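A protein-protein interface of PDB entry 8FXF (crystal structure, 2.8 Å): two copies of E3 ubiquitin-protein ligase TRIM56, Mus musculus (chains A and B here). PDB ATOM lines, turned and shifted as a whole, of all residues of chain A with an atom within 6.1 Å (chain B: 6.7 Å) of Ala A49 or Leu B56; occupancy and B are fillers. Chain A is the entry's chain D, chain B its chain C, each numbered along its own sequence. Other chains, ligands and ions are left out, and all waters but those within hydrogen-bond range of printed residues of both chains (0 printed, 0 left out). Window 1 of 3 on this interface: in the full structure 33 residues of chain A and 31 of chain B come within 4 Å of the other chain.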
ATOM      1  N   GLN A  44     -29.647  11.117 -21.562  1.00  0.00           N
ATOM      2  CA  GLN A  44     -30.869  11.127 -22.350  1.00  0.00           C
ATOM      3  C   GLN A  44     -31.006  12.467 -23.086  1.00  0.00           C
ATOM      4  O   GLN A  44     -31.489  12.549 -24.207  1.00  0.00           O
ATOM      5  CB  GLN A  44     -32.024  10.909 -21.368  1.00  0.00           C
ATOM      6  CG  GLN A  44     -33.326  10.498 -22.018  1.00  0.00           C
ATOM      7  CD  GLN A  44     -33.081   9.276 -22.865  1.00  0.00           C
ATOM      8  OE1 GLN A  44     -32.313   8.395 -22.488  1.00  0.00           O
ATOM      9  NE2 GLN A  44     -33.709   9.233 -24.029  1.00  0.00           N
ATOM     10  N   VAL A  45     -30.542  13.523 -22.431  1.00  0.00           N
ATOM     11  CA  VAL A  45     -30.531  14.874 -22.948  1.00  0.00           C
ATOM     12  C   VAL A  45     -29.422  15.036 -23.993  1.00  0.00           C
ATOM     13  O   VAL A  45     -29.717  15.467 -25.101  1.00  0.00           O
ATOM     14  CB  VAL A  45     -30.373  15.846 -21.768  1.00  0.00           C
ATOM     15  CG1 VAL A  45     -29.937  17.231 -22.214  1.00  0.00           C
ATOM     16  CG2 VAL A  45     -31.628  15.882 -20.910  1.00  0.00           C
ATOM     17  N   GLU A  46     -28.164  14.710 -23.659  1.00  0.00           N
ATOM     18  CA  GLU A  46     -27.065  14.795 -24.623  1.00  0.00           C
ATOM     19  C   GLU A  46     -27.438  14.083 -25.919  1.00  0.00           C
ATOM     20  O   GLU A  46     -27.256  14.624 -27.003  1.00  0.00           O
ATOM     21  CB  GLU A  46     -25.796  14.055 -24.196  1.00  0.00           C
ATOM     22  CG  GLU A  46     -25.217  14.515 -22.875  1.00  0.00           C
ATOM     23  CD  GLU A  46     -24.158  15.594 -22.979  1.00  0.00           C
ATOM     24  OE1 GLU A  46     -23.920  16.085 -24.097  1.00  0.00           O
ATOM     25  OE2 GLU A  46     -23.547  15.913 -21.945  1.00  0.00           O
ATOM     26  N   GLU A  47     -27.923  12.842 -25.789  1.00  0.00           N
ATOM     27  CA  GLU A  47     -28.157  11.970 -26.925  1.00  0.00           C
ATOM     28  C   GLU A  47     -29.233  12.523 -27.862  1.00  0.00           C
ATOM     29  O   GLU A  47     -28.994  12.615 -29.058  1.00  0.00           O
ATOM     30  CB  GLU A  47     -28.240  10.505 -26.489  1.00  0.00           C
ATOM     31  CG  GLU A  47     -26.862   9.998 -26.056  1.00  0.00           C
ATOM     32  CD  GLU A  47     -26.622   8.516 -25.796  1.00  0.00           C
ATOM     33  OE1 GLU A  47     -27.612   7.733 -25.710  1.00  0.00           O
ATOM     34  OE2 GLU A  47     -25.426   8.138 -25.700  1.00  0.00           O
ATOM     35  N   ALA A  48     -30.395  12.926 -27.347  1.00  0.00           N
ATOM     36  CA  ALA A  48     -31.394  13.545 -28.211  1.00  0.00           C
ATOM     37  C   ALA A  48     -30.798  14.712 -29.003  1.00  0.00           C
ATOM     38  O   ALA A  48     -31.151  14.891 -30.167  1.00  0.00           O
ATOM     39  CB  ALA A  48     -32.617  13.998 -27.440  1.00  0.00           C
ATOM     40  N   ALA A  49     -29.914  15.491 -28.358  1.00  0.00           N
ATOM     41  CA  ALA A  49     -29.257  16.654 -28.942  1.00  0.00           C
ATOM     42  C   ALA A  49     -28.361  16.246 -30.108  1.00  0.00           C
ATOM     43  O   ALA A  49     -28.276  16.968 -31.089  1.00  0.00           O
ATOM     44  CB  ALA A  49     -28.444  17.374 -27.898  1.00  0.00           C
ATOM     45  N   GLU A  50     -27.736  15.072 -30.001  1.00  0.00           N
ATOM     46  CA  GLU A  50     -26.902  14.512 -31.050  1.00  0.00           C
ATOM     47  C   GLU A  50     -27.726  13.966 -32.224  1.00  0.00           C
ATOM     48  O   GLU A  50     -27.255  14.061 -33.357  1.00  0.00           O
ATOM     49  CB  GLU A  50     -25.903  13.536 -30.435  1.00  0.00           C
ATOM     50  CG  GLU A  50     -24.913  14.249 -29.526  1.00  0.00           C
ATOM     51  CD  GLU A  50     -23.908  13.386 -28.781  1.00  0.00           C
ATOM     52  OE1 GLU A  50     -23.158  13.949 -27.949  1.00  0.00           O
ATOM     53  OE2 GLU A  50     -23.871  12.161 -29.036  1.00  0.00           O
ATOM     54  N   ARG A  51     -28.933  13.421 -31.965  1.00  0.00           N
ATOM     55  CA  ARG A  51     -29.871  12.967 -32.992  1.00  0.00           C
ATOM     56  C   ARG A  51     -30.322  14.155 -33.842  1.00  0.00           C
ATOM     57  O   ARG A  51     -30.321  14.098 -35.074  1.00  0.00           O
ATOM     58  CB  ARG A  51     -31.118  12.278 -32.408  1.00  0.00           C
ATOM     59  CG  ARG A  51     -31.039  10.754 -32.337  1.00  0.00           C
ATOM     60  CD  ARG A  51     -32.243   9.921 -31.900  1.00  0.00           C
ATOM     61  NE  ARG A  51     -31.725   8.887 -31.006  1.00  0.00           N
ATOM     62  CZ  ARG A  51     -31.693   8.976 -29.674  1.00  0.00           C
ATOM     63  NH1 ARG A  51     -32.407   9.892 -29.037  1.00  0.00           N
ATOM     64  NH2 ARG A  51     -30.950   8.134 -28.975  1.00  0.00           N
ATOM     65  N   ILE A  52     -30.720  15.227 -33.160  1.00  0.00           N
ATOM     66  CA  ILE A  52     -31.192  16.438 -33.806  1.00  0.00           C
ATOM     67  C   ILE A  52     -30.035  17.088 -34.563  1.00  0.00           C
ATOM     68  O   ILE A  52     -30.226  17.737 -35.593  1.00  0.00           O
ATOM     69  CB  ILE A  52     -31.803  17.358 -32.734  1.00  0.00           C
ATOM     70  CG1 ILE A  52     -33.163  16.814 -32.288  1.00  0.00           C
ATOM     71  CG2 ILE A  52     -31.870  18.814 -33.180  1.00  0.00           C
ATOM     72  CD1 ILE A  52     -33.646  17.374 -30.975  1.00  0.00           C
ATOM     73  N   LEU A  53     -28.822  16.912 -34.056  1.00  0.00           N
ATOM     74  CA  LEU A  53     -27.726  17.444 -34.823  1.00  0.00           C
ATOM     75  C   LEU A  53     -27.569  16.613 -36.085  1.00  0.00           C
ATOM     76  O   LEU A  53     -27.572  17.171 -37.167  1.00  0.00           O
ATOM     77  CB  LEU A  53     -26.453  17.473 -33.992  1.00  0.00           C
ATOM     78  CG  LEU A  53     -25.315  18.178 -34.713  1.00  0.00           C
ATOM     79  CD1 LEU A  53     -24.411  18.875 -33.716  1.00  0.00           C
ATOM     80  CD2 LEU A  53     -24.528  17.172 -35.526  1.00  0.00           C
ATOM     81  N   LYS A  54     -27.452  15.293 -35.929  1.00  0.00           N
ATOM     82  CA  LYS A  54     -27.326  14.368 -37.052  1.00  0.00           C
ATOM     83  C   LYS A  54     -28.403  14.606 -38.118  1.00  0.00           C
ATOM     84  O   LYS A  54     -28.093  14.676 -39.304  1.00  0.00           O
ATOM     85  CB  LYS A  54     -27.329  12.902 -36.590  1.00  0.00           C
ATOM     86  CG  LYS A  54     -26.075  12.432 -35.858  1.00  0.00           C
ATOM     87  CD  LYS A  54     -25.983  10.926 -35.695  1.00  0.00           C
ATOM     88  CE  LYS A  54     -25.285  10.530 -34.411  1.00  0.00           C
ATOM     89  NZ  LYS A  54     -25.131   9.062 -34.287  1.00  0.00           N
ATOM     90  N   ARG B  51     -29.708  28.379 -35.320  1.00  0.00           N
ATOM     91  CA  ARG B  51     -30.592  28.831 -34.258  1.00  0.00           C
ATOM     92  C   ARG B  51     -31.029  27.640 -33.408  1.00  0.00           C
ATOM     93  O   ARG B  51     -31.085  27.740 -32.183  1.00  0.00           O
ATOM     94  CB  ARG B  51     -31.770  29.647 -34.797  1.00  0.00           C
ATOM     95  CG  ARG B  51     -31.400  31.050 -35.261  1.00  0.00           C
ATOM     96  CD  ARG B  51     -32.679  31.865 -35.368  1.00  0.00           C
ATOM     97  NE  ARG B  51     -32.554  33.142 -36.047  1.00  0.00           N
ATOM     98  CZ  ARG B  51     -33.093  33.384 -37.234  1.00  0.00           C
ATOM     99  NH1 ARG B  51     -33.628  32.389 -37.925  1.00  0.00           N
ATOM    100  NH2 ARG B  51     -33.079  34.610 -37.728  1.00  0.00           N
ATOM    101  N   ILE B  52     -31.292  26.504 -34.048  1.00  0.00           N
ATOM    102  CA  ILE B  52     -31.704  25.302 -33.336  1.00  0.00           C
ATOM    103  C   ILE B  52     -30.561  24.722 -32.480  1.00  0.00           C
ATOM    104  O   ILE B  52     -30.774  24.414 -31.309  1.00  0.00           O
ATOM    105  CB  ILE B  52     -32.339  24.322 -34.343  1.00  0.00           C
ATOM    106  CG1 ILE B  52     -33.716  24.824 -34.806  1.00  0.00           C
ATOM    107  CG2 ILE B  52     -32.368  22.891 -33.832  1.00  0.00           C
ATOM    108  CD1 ILE B  52     -34.360  23.967 -35.883  1.00  0.00           C
ATOM    109  N   LEU B  53     -29.336  24.596 -33.018  1.00  0.00           N
ATOM    110  CA  LEU B  53     -28.205  24.207 -32.181  1.00  0.00           C
ATOM    111  C   LEU B  53     -27.999  25.177 -31.021  1.00  0.00           C
ATOM    112  O   LEU B  53     -27.899  24.741 -29.883  1.00  0.00           O
ATOM    113  CB  LEU B  53     -26.929  24.032 -33.008  1.00  0.00           C
ATOM    114  CG  LEU B  53     -26.576  22.587 -33.377  1.00  0.00           C
ATOM    115  CD1 LEU B  53     -27.734  21.885 -34.083  1.00  0.00           C
ATOM    116  CD2 LEU B  53     -25.315  22.536 -34.239  1.00  0.00           C
ATOM    117  N   LYS B  54     -27.969  26.482 -31.312  1.00  0.00           N
ATOM    118  CA  LYS B  54     -27.748  27.514 -30.309  1.00  0.00           C
ATOM    119  C   LYS B  54     -28.701  27.316 -29.147  1.00  0.00           C
ATOM    120  O   LYS B  54     -28.405  27.734 -28.038  1.00  0.00           O
ATOM    121  CB  LYS B  54     -27.878  28.938 -30.864  1.00  0.00           C
ATOM    122  CG  LYS B  54     -26.547  29.669 -31.017  1.00  0.00           C
ATOM    123  CD  LYS B  54     -26.469  30.738 -32.094  1.00  0.00           C
ATOM    124  CE  LYS B  54     -25.218  31.590 -31.984  1.00  0.00           C
ATOM    125  NZ  LYS B  54     -24.735  31.995 -33.326  1.00  0.00           N
ATOM    126  N   SER B  55     -29.821  26.639 -29.395  1.00  0.00           N
ATOM    127  CA  SER B  55     -30.776  26.536 -28.315  1.00  0.00           C
ATOM    128  C   SER B  55     -30.811  25.135 -27.692  1.00  0.00           C
ATOM    129  O   SER B  55     -31.166  25.006 -26.525  1.00  0.00           O
ATOM    130  CB  SER B  55     -32.108  27.145 -28.682  1.00  0.00           C
ATOM    131  OG  SER B  55     -32.921  26.207 -29.345  1.00  0.00           O
ATOM    132  N   LEU B  56     -30.405  24.090 -28.430  1.00  0.00           N
ATOM    133  CA  LEU B  56     -30.115  22.777 -27.838  1.00  0.00           C
ATOM    134  C   LEU B  56     -29.017  22.910 -26.796  1.00  0.00           C
ATOM    135  O   LEU B  56     -29.045  22.224 -25.773  1.00  0.00           O
ATOM    136  CB  LEU B  56     -29.543  21.803 -28.875  1.00  0.00           C
ATOM    137  CG  LEU B  56     -30.514  20.978 -29.708  1.00  0.00           C
ATOM    138  CD1 LEU B  56     -29.736  19.970 -30.547  1.00  0.00           C
ATOM    139  CD2 LEU B  56     -31.584  20.311 -28.832  1.00  0.00           C
ATOM    140  N   LEU B  57     -27.999  23.707 -27.147  1.00  0.00           N
ATOM    141  CA  LEU B  57     -26.808  23.827 -26.325  1.00  0.00           C
ATOM    142  C   LEU B  57     -27.145  24.612 -25.061  1.00  0.00           C
ATOM    143  O   LEU B  57     -26.745  24.228 -23.976  1.00  0.00           O
ATOM    144  CB  LEU B  57     -25.702  24.501 -27.139  1.00  0.00           C
ATOM    145  CG  LEU B  57     -25.233  23.751 -28.383  1.00  0.00           C
ATOM    146  CD1 LEU B  57     -23.757  24.033 -28.602  1.00  0.00           C
ATOM    147  CD2 LEU B  57     -25.512  22.247 -28.291  1.00  0.00           C
ATOM    148  N   ALA B  58     -27.903  25.699 -25.217  1.00  0.00           N
ATOM    149  CA  ALA B  58     -28.427  26.432 -24.083  1.00  0.00           C
ATOM    150  C   ALA B  58     -29.157  25.490 -23.117  1.00  0.00           C
ATOM    151  O   ALA B  58     -28.911  25.565 -21.926  1.00  0.00           O
ATOM    152  CB  ALA B  58     -29.279  27.581 -24.570  1.00  0.00           C
ATOM    153  N   GLN B  59     -30.044  24.619 -23.624  1.00  0.00           N
ATOM    154  CA  GLN B  59     -30.754  23.627 -22.819  1.00  0.00           C
ATOM    155  C   GLN B  59     -29.746  22.682 -22.176  1.00  0.00           C
ATOM    156  O   GLN B  59     -29.821  22.395 -20.994  1.00  0.00           O
ATOM    157  CB  GLN B  59     -31.680  22.751 -23.684  1.00  0.00           C
ATOM    158  CG  GLN B  59     -31.592  21.250 -23.349  1.00  0.00           C
ATOM    159  CD  GLN B  59     -32.330  20.224 -24.186  1.00  0.00           C
ATOM    160  OE1 GLN B  59     -33.545  20.050 -24.066  1.00  0.00           O
ATOM    161  NE2 GLN B  59     -31.623  19.619 -25.133  1.00  0.00           N
ATOM    162  N   LYS B  60     -28.816  22.166 -22.972  1.00  0.00           N
ATOM    163  CA  LYS B  60     -27.980  21.084 -22.492  1.00  0.00           C
ATOM    164  C   LYS B  60     -27.216  21.610 -21.287  1.00  0.00           C
ATOM    165  O   LYS B  60     -27.058  20.919 -20.294  1.00  0.00           O
ATOM    166  CB  LYS B  60     -26.961  20.722 -23.572  1.00  0.00           C
ATOM    167  CG  LYS B  60     -26.657  19.249 -23.762  1.00  0.00           C
ATOM    168  CD  LYS B  60     -25.498  19.049 -24.712  1.00  0.00           C
ATOM    169  CE  LYS B  60     -24.180  19.462 -24.103  1.00  0.00           C
ATOM    170  NZ  LYS B  60     -23.084  19.286 -25.085  1.00  0.00           N
ATOM    171  N   GLN B  61     -26.783  22.869 -21.371  1.00  0.00           N
ATOM    172  CA  GLN B  61     -25.981  23.461 -20.320  1.00  0.00           C
ATOM    173  C   GLN B  61     -26.836  23.730 -19.076  1.00  0.00           C
ATOM    174  O   GLN B  61     -26.546  23.257 -17.984  1.00  0.00           O
ATOM    175  CB  GLN B  61     -25.391  24.748 -20.855  1.00  0.00           C
ATOM    176  CG  GLN B  61     -23.993  25.005 -20.339  1.00  0.00           C
ATOM    177  CD  GLN B  61     -23.586  26.392 -20.759  1.00  0.00           C
ATOM    178  OE1 GLN B  61     -23.540  26.706 -21.950  1.00  0.00           O
ATOM    179  NE2 GLN B  61     -23.312  27.235 -19.774  1.00  0.00           N
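Of the 11 printed residues of chain B, 3 touch a printed residue of chain A. Hydrophobic or aromatic side chains of chain B within 4 Å of the printed part of chain A: Leu B53 and Leu B56. Hydrophobic or aromatic side chains of chain A that line the printed part of chain B: Ala A49, Ile A52 and Leu A53.
The side-chain carboxylate (OE1) of Glu A46 is in salt-bridge range of the side-chain amino group (NZ) of Lys B60 (3.5 Å).
Leu B53 touches its own counterpart, Leu A53.
Among the printed residues, pairs that only touch across the chains: Ala A49 with Leu B56 (3.4 Å), Ile A52 with Leu B56 (3.6 Å) and Leu A53 with Leu B53 (3.8 Å).
Ala A49 touches just one residue of chain B: Leu B56. Of the printed residues of chain B, Leu A53 touches Leu B53 (3.8 Å). Of the printed residues of chain A, Leu B53 touches Leu A53 (3.8 Å). Of the printed residues of chain B, Glu A46 touches Lys B60. Ala B58 touches none of the printed residues of chain A. The nearest residue of chain A that does not touch Leu B56 is Leu A53 (4.7 Å).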
